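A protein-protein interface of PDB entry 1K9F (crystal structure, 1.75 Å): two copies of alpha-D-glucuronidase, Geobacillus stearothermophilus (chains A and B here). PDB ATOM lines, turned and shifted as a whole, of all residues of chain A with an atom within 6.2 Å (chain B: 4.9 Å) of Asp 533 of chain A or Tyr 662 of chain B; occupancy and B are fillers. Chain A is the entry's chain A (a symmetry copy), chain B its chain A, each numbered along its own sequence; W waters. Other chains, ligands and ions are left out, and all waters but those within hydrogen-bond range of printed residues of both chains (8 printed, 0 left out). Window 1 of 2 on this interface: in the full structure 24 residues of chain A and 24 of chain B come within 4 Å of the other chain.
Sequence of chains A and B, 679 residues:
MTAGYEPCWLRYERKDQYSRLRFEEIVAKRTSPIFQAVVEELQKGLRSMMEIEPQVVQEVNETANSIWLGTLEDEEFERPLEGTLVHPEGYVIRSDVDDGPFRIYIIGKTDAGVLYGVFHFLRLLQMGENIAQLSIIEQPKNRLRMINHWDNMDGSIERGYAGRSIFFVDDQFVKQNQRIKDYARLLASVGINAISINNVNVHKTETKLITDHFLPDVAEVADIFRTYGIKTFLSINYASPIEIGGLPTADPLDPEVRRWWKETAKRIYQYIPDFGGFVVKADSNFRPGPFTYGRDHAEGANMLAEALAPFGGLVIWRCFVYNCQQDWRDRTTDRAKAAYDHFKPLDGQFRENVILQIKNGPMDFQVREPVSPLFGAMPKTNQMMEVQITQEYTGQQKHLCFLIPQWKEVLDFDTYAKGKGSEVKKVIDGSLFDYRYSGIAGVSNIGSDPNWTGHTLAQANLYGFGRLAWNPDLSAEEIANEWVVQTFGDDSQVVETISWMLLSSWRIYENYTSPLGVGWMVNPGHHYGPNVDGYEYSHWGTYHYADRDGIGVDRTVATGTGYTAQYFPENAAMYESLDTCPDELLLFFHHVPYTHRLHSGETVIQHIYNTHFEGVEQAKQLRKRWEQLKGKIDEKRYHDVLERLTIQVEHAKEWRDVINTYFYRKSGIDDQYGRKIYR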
ATOM      1  N   MET A 521       2.539  -6.305   0.572  1.00  0.00           N
ATOM      2  CA  MET A 521       3.391  -7.286  -0.105  1.00  0.00           C
ATOM      3  C   MET A 521       2.545  -8.124  -1.075  1.00  0.00           C
ATOM      4  O   MET A 521       2.833  -9.299  -1.323  1.00  0.00           O
ATOM      5  CB  MET A 521       4.098  -8.197   0.907  1.00  0.00           C
ATOM      6  CG  MET A 521       5.094  -7.451   1.796  1.00  0.00           C
ATOM      7  SD  MET A 521       6.175  -8.558   2.723  1.00  0.00           S
ATOM      8  CE  MET A 521       7.171  -7.381   3.616  1.00  0.00           C
ATOM      9  N   VAL A 522       1.504  -7.501  -1.626  1.00  0.00           N
ATOM     10  CA  VAL A 522       0.606  -8.160  -2.577  1.00  0.00           C
ATOM     11  C   VAL A 522       0.736  -7.581  -3.984  1.00  0.00           C
ATOM     12  O   VAL A 522       1.242  -6.469  -4.171  1.00  0.00           O
ATOM     13  CB  VAL A 522      -0.888  -8.008  -2.168  1.00  0.00           C
ATOM     14  CG1 VAL A 522      -1.163  -8.740  -0.862  1.00  0.00           C
ATOM     15  CG2 VAL A 522      -1.243  -6.531  -2.039  1.00  0.00           C
ATOM     16  N   PRO A 524      -0.172  -5.603  -7.145  1.00  0.00           N
ATOM     17  CA  PRO A 524      -1.000  -4.404  -7.295  1.00  0.00           C
ATOM     18  C   PRO A 524      -2.239  -4.687  -8.136  1.00  0.00           C
ATOM     19  O   PRO A 524      -2.254  -5.622  -8.936  1.00  0.00           O
ATOM     20  CB  PRO A 524      -0.061  -3.414  -7.986  1.00  0.00           C
ATOM     21  CG  PRO A 524       1.308  -3.870  -7.548  1.00  0.00           C
ATOM     22  CD  PRO A 524       1.193  -5.370  -7.653  1.00  0.00           C
ATOM     23  N   ASN A 531       4.100 -10.196  -3.837  1.00  0.00           N
ATOM     24  CA  ASN A 531       4.799  -9.187  -4.621  1.00  0.00           C
ATOM     25  C   ASN A 531       5.256  -8.207  -3.551  1.00  0.00           C
ATOM     26  O   ASN A 531       4.604  -7.191  -3.300  1.00  0.00           O
ATOM     27  CB  ASN A 531       3.853  -8.492  -5.603  1.00  0.00           C
ATOM     28  CG  ASN A 531       4.599  -7.680  -6.637  1.00  0.00           C
ATOM     29  OD1 ASN A 531       5.647  -7.105  -6.344  1.00  0.00           O
ATOM     30  ND2 ASN A 531       4.061  -7.620  -7.854  1.00  0.00           N
ATOM     31  N   VAL A 532       6.373  -8.531  -2.907  1.00  0.00           N
ATOM     32  CA  VAL A 532       6.886  -7.717  -1.817  1.00  0.00           C
ATOM     33  C   VAL A 532       6.970  -6.225  -2.102  1.00  0.00           C
ATOM     34  O   VAL A 532       6.547  -5.418  -1.271  1.00  0.00           O
ATOM     35  CB  VAL A 532       8.257  -8.229  -1.341  1.00  0.00           C
ATOM     36  CG1 VAL A 532       8.763  -7.369  -0.183  1.00  0.00           C
ATOM     37  CG2 VAL A 532       8.129  -9.681  -0.889  1.00  0.00           C
ATOM     38  N   ASP A 533       7.501  -5.853  -3.265  1.00  0.00           N
ATOM     39  CA  ASP A 533       7.620  -4.440  -3.627  1.00  0.00           C
ATOM     40  C   ASP A 533       6.450  -3.921  -4.466  1.00  0.00           C
ATOM     41  O   ASP A 533       6.519  -2.828  -5.018  1.00  0.00           O
ATOM     42  CB  ASP A 533       8.932  -4.196  -4.387  1.00  0.00           C
ATOM     43  CG  ASP A 533      10.124  -4.002  -3.461  1.00  0.00           C
ATOM     44  OD1 ASP A 533       9.993  -4.233  -2.239  1.00  0.00           O
ATOM     45  OD2 ASP A 533      11.202  -3.615  -3.959  1.00  0.00           O
ATOM     46  N   GLY A 534       5.376  -4.702  -4.543  1.00  0.00           N
ATOM     47  CA  GLY A 534       4.209  -4.316  -5.322  1.00  0.00           C
ATOM     48  C   GLY A 534       3.825  -2.842  -5.278  1.00  0.00           C
ATOM     49  O   GLY A 534       3.745  -2.181  -6.317  1.00  0.00           O
ATOM     50  N   TYR A 535       3.588  -2.325  -4.079  1.00  0.00           N
ATOM     51  CA  TYR A 535       3.206  -0.925  -3.906  1.00  0.00           C
ATOM     52  C   TYR A 535       4.291  -0.124  -3.187  1.00  0.00           C
ATOM     53  O   TYR A 535       4.053   1.017  -2.781  1.00  0.00           O
ATOM     54  CB  TYR A 535       1.913  -0.835  -3.084  1.00  0.00           C
ATOM     55  CG  TYR A 535       0.636  -1.174  -3.828  1.00  0.00           C
ATOM     56  CD1 TYR A 535       0.190  -0.380  -4.883  1.00  0.00           C
ATOM     57  CD2 TYR A 535      -0.152  -2.259  -3.443  1.00  0.00           C
ATOM     58  CE1 TYR A 535      -1.009  -0.650  -5.533  1.00  0.00           C
ATOM     59  CE2 TYR A 535      -1.355  -2.543  -4.087  1.00  0.00           C
ATOM     60  CZ  TYR A 535      -1.777  -1.730  -5.133  1.00  0.00           C
ATOM     61  OH  TYR A 535      -2.963  -1.987  -5.771  1.00  0.00           O
ATOM     62  N   GLU A 536       5.481  -0.709  -3.060  1.00  0.00           N
ATOM     63  CA  GLU A 536       6.587  -0.076  -2.338  1.00  0.00           C
ATOM     64  C   GLU A 536       7.047   1.295  -2.844  1.00  0.00           C
ATOM     65  O   GLU A 536       7.581   2.086  -2.068  1.00  0.00           O
ATOM     66  CB  GLU A 536       7.773  -1.053  -2.264  1.00  0.00           C
ATOM     67  CG  GLU A 536       8.923  -0.627  -1.350  1.00  0.00           C
ATOM     68  CD  GLU A 536       8.516  -0.426   0.106  1.00  0.00           C
ATOM     69  OE1 GLU A 536       7.401  -0.840   0.496  1.00  0.00           O
ATOM     70  OE2 GLU A 536       9.327   0.145   0.868  1.00  0.00           O
ATOM     71  N   TYR A 537       6.851   1.581  -4.128  1.00  0.00           N
ATOM     72  CA  TYR A 537       7.228   2.888  -4.666  1.00  0.00           C
ATOM     73  C   TYR A 537       6.021   3.568  -5.298  1.00  0.00           C
ATOM     74  O   TYR A 537       6.151   4.426  -6.174  1.00  0.00           O
ATOM     75  CB  TYR A 537       8.362   2.746  -5.686  1.00  0.00           C
ATOM     76  CG  TYR A 537       9.622   2.178  -5.074  1.00  0.00           C
ATOM     77  CD1 TYR A 537       9.803   0.802  -4.959  1.00  0.00           C
ATOM     78  CD2 TYR A 537      10.611   3.020  -4.559  1.00  0.00           C
ATOM     79  CE1 TYR A 537      10.939   0.272  -4.345  1.00  0.00           C
ATOM     80  CE2 TYR A 537      11.750   2.500  -3.941  1.00  0.00           C
ATOM     81  CZ  TYR A 537      11.906   1.126  -3.836  1.00  0.00           C
ATOM     82  OH  TYR A 537      13.016   0.604  -3.208  1.00  0.00           O
ATOM     83  N   HIS A 544       6.929  -0.667   3.344  1.00  0.00           N
ATOM     84  CA  HIS A 544       7.559  -1.463   4.394  1.00  0.00           C
ATOM     85  C   HIS A 544       9.010  -1.015   4.617  1.00  0.00           C
ATOM     86  O   HIS A 544       9.628  -1.355   5.630  1.00  0.00           O
ATOM     87  CB  HIS A 544       7.497  -2.961   4.053  1.00  0.00           C
ATOM     88  CG  HIS A 544       8.046  -3.304   2.703  1.00  0.00           C
ATOM     89  ND1 HIS A 544       9.362  -3.088   2.358  1.00  0.00           N
ATOM     90  CD2 HIS A 544       7.454  -3.843   1.610  1.00  0.00           C
ATOM     91  CE1 HIS A 544       9.558  -3.477   1.111  1.00  0.00           C
ATOM     92  NE2 HIS A 544       8.416  -3.939   0.633  1.00  0.00           N
ATOM     93  N   ALA A 546      11.817  -1.936   3.408  1.00  0.00           N
ATOM     94  CA  ALA A 546      12.848  -2.953   3.544  1.00  0.00           C
ATOM     95  C   ALA A 546      14.099  -2.594   2.743  1.00  0.00           C
ATOM     96  O   ALA A 546      14.013  -2.146   1.596  1.00  0.00           O
ATOM     97  CB  ALA A 546      12.317  -4.299   3.082  1.00  0.00           C
ATOM     98  N   TYR A 662      13.006 -13.013  -1.542  1.00  0.00           N
ATOM     99  CA  TYR A 662      13.150 -11.563  -1.518  1.00  0.00           C
ATOM    100  C   TYR A 662      13.978 -11.129  -0.321  1.00  0.00           C
ATOM    101  O   TYR A 662      14.868 -10.285  -0.437  1.00  0.00           O
ATOM    102  CB  TYR A 662      11.775 -10.882  -1.461  1.00  0.00           C
ATOM    103  CG  TYR A 662      11.837  -9.371  -1.324  1.00  0.00           C
ATOM    104  CD1 TYR A 662      12.133  -8.768  -0.097  1.00  0.00           C
ATOM    105  CD2 TYR A 662      11.605  -8.543  -2.423  1.00  0.00           C
ATOM    106  CE1 TYR A 662      12.194  -7.378   0.027  1.00  0.00           C
ATOM    107  CE2 TYR A 662      11.665  -7.148  -2.307  1.00  0.00           C
ATOM    108  CZ  TYR A 662      11.959  -6.576  -1.079  1.00  0.00           C
ATOM    109  OH  TYR A 662      12.009  -5.204  -0.955  1.00  0.00           O
ATOM    110  N   LYS A 666      17.843  -9.661  -0.038  1.00  0.00           N
ATOM    111  CA  LYS A 666      18.111  -8.370   0.579  1.00  0.00           C
ATOM    112  C   LYS A 666      18.937  -8.454   1.869  1.00  0.00           C
ATOM    113  O   LYS A 666      19.852  -7.654   2.073  1.00  0.00           O
ATOM    114  CB  LYS A 666      16.789  -7.639   0.848  1.00  0.00           C
ATOM    115  CG  LYS A 666      16.883  -6.141   0.652  1.00  0.00           C
ATOM    116  CD  LYS A 666      15.513  -5.488   0.523  1.00  0.00           C
ATOM    117  CE  LYS A 666      15.564  -4.412  -0.549  1.00  0.00           C
ATOM    118  NZ  LYS A 666      14.301  -3.639  -0.677  1.00  0.00           N
ATOM    119  N   ASN B 531       9.318   0.351 -11.643  1.00  0.00           N
ATOM    120  CA  ASN B 531       8.886  -0.676 -10.706  1.00  0.00           C
ATOM    121  C   ASN B 531       9.936  -1.760 -10.908  1.00  0.00           C
ATOM    122  O   ASN B 531       9.724  -2.716 -11.656  1.00  0.00           O
ATOM    123  CB  ASN B 531       7.499  -1.212 -11.068  1.00  0.00           C
ATOM    124  CG  ASN B 531       6.894  -2.034  -9.952  1.00  0.00           C
ATOM    125  OD1 ASN B 531       7.609  -2.728  -9.230  1.00  0.00           O
ATOM    126  ND2 ASN B 531       5.573  -1.967  -9.807  1.00  0.00           N
ATOM    127  N   VAL B 532      11.078  -1.589 -10.250  1.00  0.00           N
ATOM    128  CA  VAL B 532      12.189  -2.514 -10.404  1.00  0.00           C
ATOM    129  C   VAL B 532      11.833  -3.988 -10.276  1.00  0.00           C
ATOM    130  O   VAL B 532      12.256  -4.795 -11.107  1.00  0.00           O
ATOM    131  CB  VAL B 532      13.332  -2.174  -9.431  1.00  0.00           C
ATOM    132  CG1 VAL B 532      14.494  -3.148  -9.629  1.00  0.00           C
ATOM    133  CG2 VAL B 532      13.807  -0.745  -9.684  1.00  0.00           C
ATOM    134  N   ASP B 533      11.056  -4.343  -9.255  1.00  0.00           N
ATOM    135  CA  ASP B 533      10.657  -5.737  -9.053  1.00  0.00           C
ATOM    136  C   ASP B 533       9.301  -6.083  -9.670  1.00  0.00           C
ATOM    137  O   ASP B 533       8.748  -7.143  -9.398  1.00  0.00           O
ATOM    138  CB  ASP B 533      10.629  -6.068  -7.554  1.00  0.00           C
ATOM    139  CG  ASP B 533      11.999  -6.438  -7.004  1.00  0.00           C
ATOM    140  OD1 ASP B 533      13.011  -6.266  -7.718  1.00  0.00           O
ATOM    141  OD2 ASP B 533      12.065  -6.903  -5.847  1.00  0.00           O
ATOM    142  N   HIS B 544      15.939  -9.823 -13.380  1.00  0.00           N
ATOM    143  CA  HIS B 544      17.238  -9.159 -13.318  1.00  0.00           C
ATOM    144  C   HIS B 544      18.105  -9.766 -12.206  1.00  0.00           C
ATOM    145  O   HIS B 544      19.319  -9.551 -12.163  1.00  0.00           O
ATOM    146  CB  HIS B 544      17.066  -7.645 -13.111  1.00  0.00           C
ATOM    147  CG  HIS B 544      16.210  -7.281 -11.938  1.00  0.00           C
ATOM    148  ND1 HIS B 544      16.544  -7.610 -10.643  1.00  0.00           N
ATOM    149  CD2 HIS B 544      15.029  -6.621 -11.867  1.00  0.00           C
ATOM    150  CE1 HIS B 544      15.606  -7.170  -9.823  1.00  0.00           C
ATOM    151  NE2 HIS B 544      14.674  -6.567 -10.540  1.00  0.00           N
ATOM    152  N   ALA B 546      18.550  -9.067  -9.123  1.00  0.00           N
ATOM    153  CA  ALA B 546      19.282  -8.170  -8.243  1.00  0.00           C
ATOM    154  C   ALA B 546      19.176  -8.607  -6.782  1.00  0.00           C
ATOM    155  O   ALA B 546      18.099  -8.976  -6.305  1.00  0.00           O
ATOM    156  CB  ALA B 546      18.758  -6.753  -8.388  1.00  0.00           C
ATOM    157  N   ASP B 657      14.641   8.570  -9.164  1.00  0.00           N
ATOM    158  CA  ASP B 657      14.596   8.311  -7.737  1.00  0.00           C
ATOM    159  C   ASP B 657      14.194   6.889  -7.358  1.00  0.00           C
ATOM    160  O   ASP B 657      14.781   6.308  -6.452  1.00  0.00           O
ATOM    161  CB  ASP B 657      13.691   9.335  -7.040  1.00  0.00           C
ATOM    162  CG  ASP B 657      14.216  10.765  -7.172  1.00  0.00           C
ATOM    163  OD1 ASP B 657      15.441  10.948  -7.379  1.00  0.00           O
ATOM    164  OD2 ASP B 657      13.407  11.711  -7.057  1.00  0.00           O
ATOM    165  N   VAL B 658      13.207   6.322  -8.042  1.00  0.00           N
ATOM    166  CA  VAL B 658      12.792   4.962  -7.719  1.00  0.00           C
ATOM    167  C   VAL B 658      13.952   3.987  -7.938  1.00  0.00           C
ATOM    168  O   VAL B 658      14.273   3.182  -7.060  1.00  0.00           O
ATOM    169  CB  VAL B 658      11.574   4.520  -8.568  1.00  0.00           C
ATOM    170  CG1 VAL B 658      11.300   3.037  -8.351  1.00  0.00           C
ATOM    171  CG2 VAL B 658      10.342   5.331  -8.168  1.00  0.00           C
ATOM    172  N   ILE B 659      14.594   4.065  -9.101  1.00  0.00           N
ATOM    173  CA  ILE B 659      15.706   3.167  -9.383  1.00  0.00           C
ATOM    174  C   ILE B 659      16.888   3.403  -8.445  1.00  0.00           C
ATOM    175  O   ILE B 659      17.438   2.450  -7.895  1.00  0.00           O
ATOM    176  CB  ILE B 659      16.150   3.277 -10.868  1.00  0.00           C
ATOM    177  CG1 ILE B 659      15.069   2.636 -11.751  1.00  0.00           C
ATOM    178  CG2 ILE B 659      17.499   2.578 -11.078  1.00  0.00           C
ATOM    179  CD1 ILE B 659      15.338   2.693 -13.239  1.00  0.00           C
ATOM    180  N   ASN B 660      17.271   4.660  -8.244  1.00  0.00           N
ATOM    181  CA  ASN B 660      18.391   4.950  -7.352  1.00  0.00           C
ATOM    182  C   ASN B 660      18.129   4.460  -5.930  1.00  0.00           C
ATOM    183  O   ASN B 660      19.000   3.855  -5.306  1.00  0.00           O
ATOM    184  CB  ASN B 660      18.693   6.453  -7.316  1.00  0.00           C
ATOM    185  CG  ASN B 660      19.383   6.940  -8.574  1.00  0.00           C
ATOM    186  OD1 ASN B 660      19.881   6.144  -9.371  1.00  0.00           O
ATOM    187  ND2 ASN B 660      19.433   8.259  -8.751  1.00  0.00           N
ATOM    188  N   THR B 661      16.934   4.724  -5.411  1.00  0.00           N
ATOM    189  CA  THR B 661      16.604   4.287  -4.058  1.00  0.00           C
ATOM    190  C   THR B 661      16.581   2.766  -3.958  1.00  0.00           C
ATOM    191  O   THR B 661      17.088   2.192  -2.995  1.00  0.00           O
ATOM    192  CB  THR B 661      15.244   4.850  -3.602  1.00  0.00           C
ATOM    193  OG1 THR B 661      15.351   6.271  -3.444  1.00  0.00           O
ATOM    194  CG2 THR B 661      14.818   4.223  -2.270  1.00  0.00           C
ATOM    195  N   TYR B 662      16.005   2.103  -4.954  1.00  0.00           N
ATOM    196  CA  TYR B 662      15.949   0.647  -4.927  1.00  0.00           C
ATOM    197  C   TYR B 662      17.347   0.061  -4.842  1.00  0.00           C
ATOM    198  O   TYR B 662      17.602  -0.861  -4.066  1.00  0.00           O
ATOM    199  CB  TYR B 662      15.246   0.108  -6.182  1.00  0.00           C
ATOM    200  CG  TYR B 662      15.240  -1.407  -6.287  1.00  0.00           C
ATOM    201  CD1 TYR B 662      16.383  -2.109  -6.684  1.00  0.00           C
ATOM    202  CD2 TYR B 662      14.093  -2.141  -5.982  1.00  0.00           C
ATOM    203  CE1 TYR B 662      16.379  -3.502  -6.776  1.00  0.00           C
ATOM    204  CE2 TYR B 662      14.080  -3.539  -6.071  1.00  0.00           C
ATOM    205  CZ  TYR B 662      15.226  -4.210  -6.469  1.00  0.00           C
ATOM    206  OH  TYR B 662      15.217  -5.585  -6.569  1.00  0.00           O
ATOM    207  N   PHE B 663      18.264   0.592  -5.640  1.00  0.00           N
ATOM    208  CA  PHE B 663      19.613   0.059  -5.633  1.00  0.00           C
ATOM    209  C   PHE B 663      20.451   0.506  -4.457  1.00  0.00           C
ATOM    210  O   PHE B 663      21.388  -0.189  -4.068  1.00  0.00           O
ATOM    211  CB  PHE B 663      20.273   0.326  -6.982  1.00  0.00           C
ATOM    212  CG  PHE B 663      19.770  -0.598  -8.048  1.00  0.00           C
ATOM    213  CD1 PHE B 663      20.089  -1.956  -8.003  1.00  0.00           C
ATOM    214  CD2 PHE B 663      18.879  -0.155  -9.014  1.00  0.00           C
ATOM    215  CE1 PHE B 663      19.519  -2.858  -8.898  1.00  0.00           C
ATOM    216  CE2 PHE B 663      18.303  -1.049  -9.916  1.00  0.00           C
ATOM    217  CZ  PHE B 663      18.621  -2.402  -9.857  1.00  0.00           C
ATOM    218  N   TYR B 664      20.118   1.651  -3.872  1.00  0.00           N
ATOM    219  CA  TYR B 664      20.846   2.069  -2.682  1.00  0.00           C
ATOM    220  C   TYR B 664      20.363   1.154  -1.549  1.00  0.00           C
ATOM    221  O   TYR B 664      21.155   0.648  -0.750  1.00  0.00           O
ATOM    222  CB  TYR B 664      20.549   3.520  -2.310  1.00  0.00           C
ATOM    223  CG  TYR B 664      21.141   3.875  -0.966  1.00  0.00           C
ATOM    224  CD1 TYR B 664      22.523   3.972  -0.795  1.00  0.00           C
ATOM    225  CD2 TYR B 664      20.327   4.027   0.156  1.00  0.00           C
ATOM    226  CE1 TYR B 664      23.083   4.202   0.464  1.00  0.00           C
ATOM    227  CE2 TYR B 664      20.873   4.259   1.419  1.00  0.00           C
ATOM    228  CZ  TYR B 664      22.251   4.341   1.565  1.00  0.00           C
ATOM    229  OH  TYR B 664      22.793   4.538   2.816  1.00  0.00           O
ATOM    230  N   ARG B 665      19.054   0.930  -1.486  1.00  0.00           N
ATOM    231  CA  ARG B 665      18.506   0.070  -0.446  1.00  0.00           C
ATOM    232  C   ARG B 665      19.063  -1.344  -0.528  1.00  0.00           C
ATOM    233  O   ARG B 665      19.237  -1.999   0.493  1.00  0.00           O
ATOM    234  CB  ARG B 665      16.980   0.030  -0.519  1.00  0.00           C
ATOM    235  CG  ARG B 665      16.330   1.289   0.024  1.00  0.00           C
ATOM    236  CD  ARG B 665      14.810   1.222  -0.037  1.00  0.00           C
ATOM    237  NE  ARG B 665      14.214   2.455   0.472  1.00  0.00           N
ATOM    238  CZ  ARG B 665      12.942   2.799   0.294  1.00  0.00           C
ATOM    239  NH1 ARG B 665      12.127   2.003  -0.380  1.00  0.00           N
ATOM    240  NH2 ARG B 665      12.487   3.945   0.780  1.00  0.00           N
ATOM    241  N   LYS B 666      19.360  -1.809  -1.739  1.00  0.00           N
ATOM    242  CA  LYS B 666      19.892  -3.154  -1.894  1.00  0.00           C
ATOM    243  C   LYS B 666      21.423  -3.232  -1.826  1.00  0.00           C
ATOM    244  O   LYS B 666      21.971  -4.131  -1.187  1.00  0.00           O
ATOM    245  CB  LYS B 666      19.393  -3.761  -3.212  1.00  0.00           C
ATOM    246  CG  LYS B 666      19.118  -5.247  -3.121  1.00  0.00           C
ATOM    247  CD  LYS B 666      18.260  -5.748  -4.275  1.00  0.00           C
ATOM    248  CE  LYS B 666      17.251  -6.758  -3.756  1.00  0.00           C
ATOM    249  NZ  LYS B 666      16.435  -7.389  -4.826  1.00  0.00           N
HETATM  250  O   HOH W   1       9.364  -7.624  -4.940  1.00  0.00           O
HETATM  251  O   HOH W   2       8.009  -1.564  -6.918  1.00  0.00           O
HETATM  252  O   HOH W   3       7.720  -8.439  -7.230  1.00  0.00           O
HETATM  253  O   HOH W   4      11.870  -1.022   0.148  1.00  0.00           O
HETATM  254  O   HOH W   5      10.717  -2.676  -6.702  1.00  0.00           O
HETATM  255  O   HOH W   6      15.802  -2.683  -3.104  1.00  0.00           O
HETATM  256  O   HOH W   7      14.990  -8.349  -2.366  1.00  0.00           O
HETATM  257  O   HOH W   8       9.388   2.877  -0.092  1.00  0.00           O
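The guanidinium group (NH1) of Arg 665 of chain B is in salt-bridge range of the side-chain carboxylate (OE2) of Glu 536 of chain A (3.6 Å). The side-chain hydroxyl (OH) of Tyr 537 of chain A sits at hydrogen-bond distance from the guanidinium group (NH1) of Arg 665 of chain B.
The side-chain hydroxyl (OH) of Tyr 662 of chain B is in hydrogen-bond range of the side-chain carboxylate (OD1) of Asp 533 of chain B, 2.6 Å away. The side-chain amide oxygen (OD1) of Asn 531 of chain A sits at hydrogen-bond distance from the backbone NH (N) of Gly 534 of chain A (3.0 Å). The side-chain carboxylate (OD1) of Asp 533 of chain A lies within hydrogen-bond range of a ring nitrogen (NE2) of His 544 of chain A (3.3 Å). OD1 of Asp 533 of chain A sits at hydrogen-bond distance from OH of Tyr 662 of chain A (2.6 Å). OE1 of Glu 536 of chain A is in hydrogen-bond range of N of His 544 of chain A (2.9 Å). The side-chain amino group (NZ) of Lys 666 of chain A is in hydrogen-bond range of the backbone carbonyl oxygen (O) of Ala 546 of chain A (2.7 Å).
Among the printed residues, merely in contact across the chains: Asp 533 of chain A with Asp 533 of chain B, Asp 533 of chain A with Tyr 662 of chain B, Gly 534 of chain A with Asn 531 of chain B, Tyr 537 of chain A with Val 658 of chain B, Tyr 537 of chain A with Thr 661 of chain B, Tyr 537 of chain A with Tyr 662 of chain B, Ala 546 of chain A with Arg 665 of chain B and Tyr 662 of chain A with Asp 533 of chain B.
Of chain B, only Asp 533 (3.9 Å) and Tyr 662 (3.6 Å) come within 4 Å of Asp 533 of chain A. Of the printed residues of chain B, Tyr 537 of chain A touches Val 658 (3.8 Å), Thr 661 (3.9 Å), Tyr 662 (3.4 Å) and Arg 665 (3.3 Å). Printed residues of chain B within 4 Å of Tyr 662 of chain A: Asp 533 (3.6 Å). Asn 531 of chain A touches none of the printed residues of chain B. Tyr 664 of chain B touches none of the printed residues of chain A. The nearest printed residue of chain A that does not touch Arg 665 of chain B is Lys 666 of chain A (4.5 Å).
Of the 14 printed residues of chain A, 6 touch a printed residue of chain B. Printed residues of chain A that touch a printed residue of chain B: Asp 533, Gly 534, Glu 536, Tyr 537, Ala 546 and Tyr 662. Hydrophobic or aromatic side chains of chain A that line the printed part of chain B: Tyr 537 and Tyr 662. Printed residues of chain B that touch a printed residue of chain A: Asn 531, Asp 533, Val 658, Thr 661, Tyr 662 and Arg 665. Among the printed residues, 10 pairs touch across the chains.
Asp 533 of chain B touches its own counterpart, Asp 533 of chain A. Asp 533 of chain A touches Tyr 662 of chain B, and with the chains exchanged Tyr 662 of chain A touches Asp 533 of chain B. Positions printed for both chains: 531, 532, 533, 544, 546, 662 and 666. Of the 10 pairs that touch across the chains among the printed residues, 3 have their exchanged pair printed and touching as well.
Water W3 bridges OD1 of Asn 531 of chain A (2.6 Å) and O of Asp 533 of chain B (2.7 Å). Water W2 lies within hydrogen-bond range of the side-chain amide oxygen (OD1) of Asn 531 of chain B and the backbone carbonyl oxygen (O) of Asp 533 of chain A. Water W7 bridges O of Tyr 662 of chain A and NZ of Lys 666 of chain B. Water W6 bridges O of Tyr 662 of chain B (2.7 Å) and NZ of Lys 666 of chain A (3.0 Å). Water W4 lies within hydrogen-bond range of the backbone carbonyl oxygen of Ala 546 of chain A, the side-chain carboxylate of Glu 536 of chain A and the guanidinium group of Arg 665 of chain B. Water W1 bridges OD2 of Asp 533 of chain B and N of Asp 533 of chain A.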
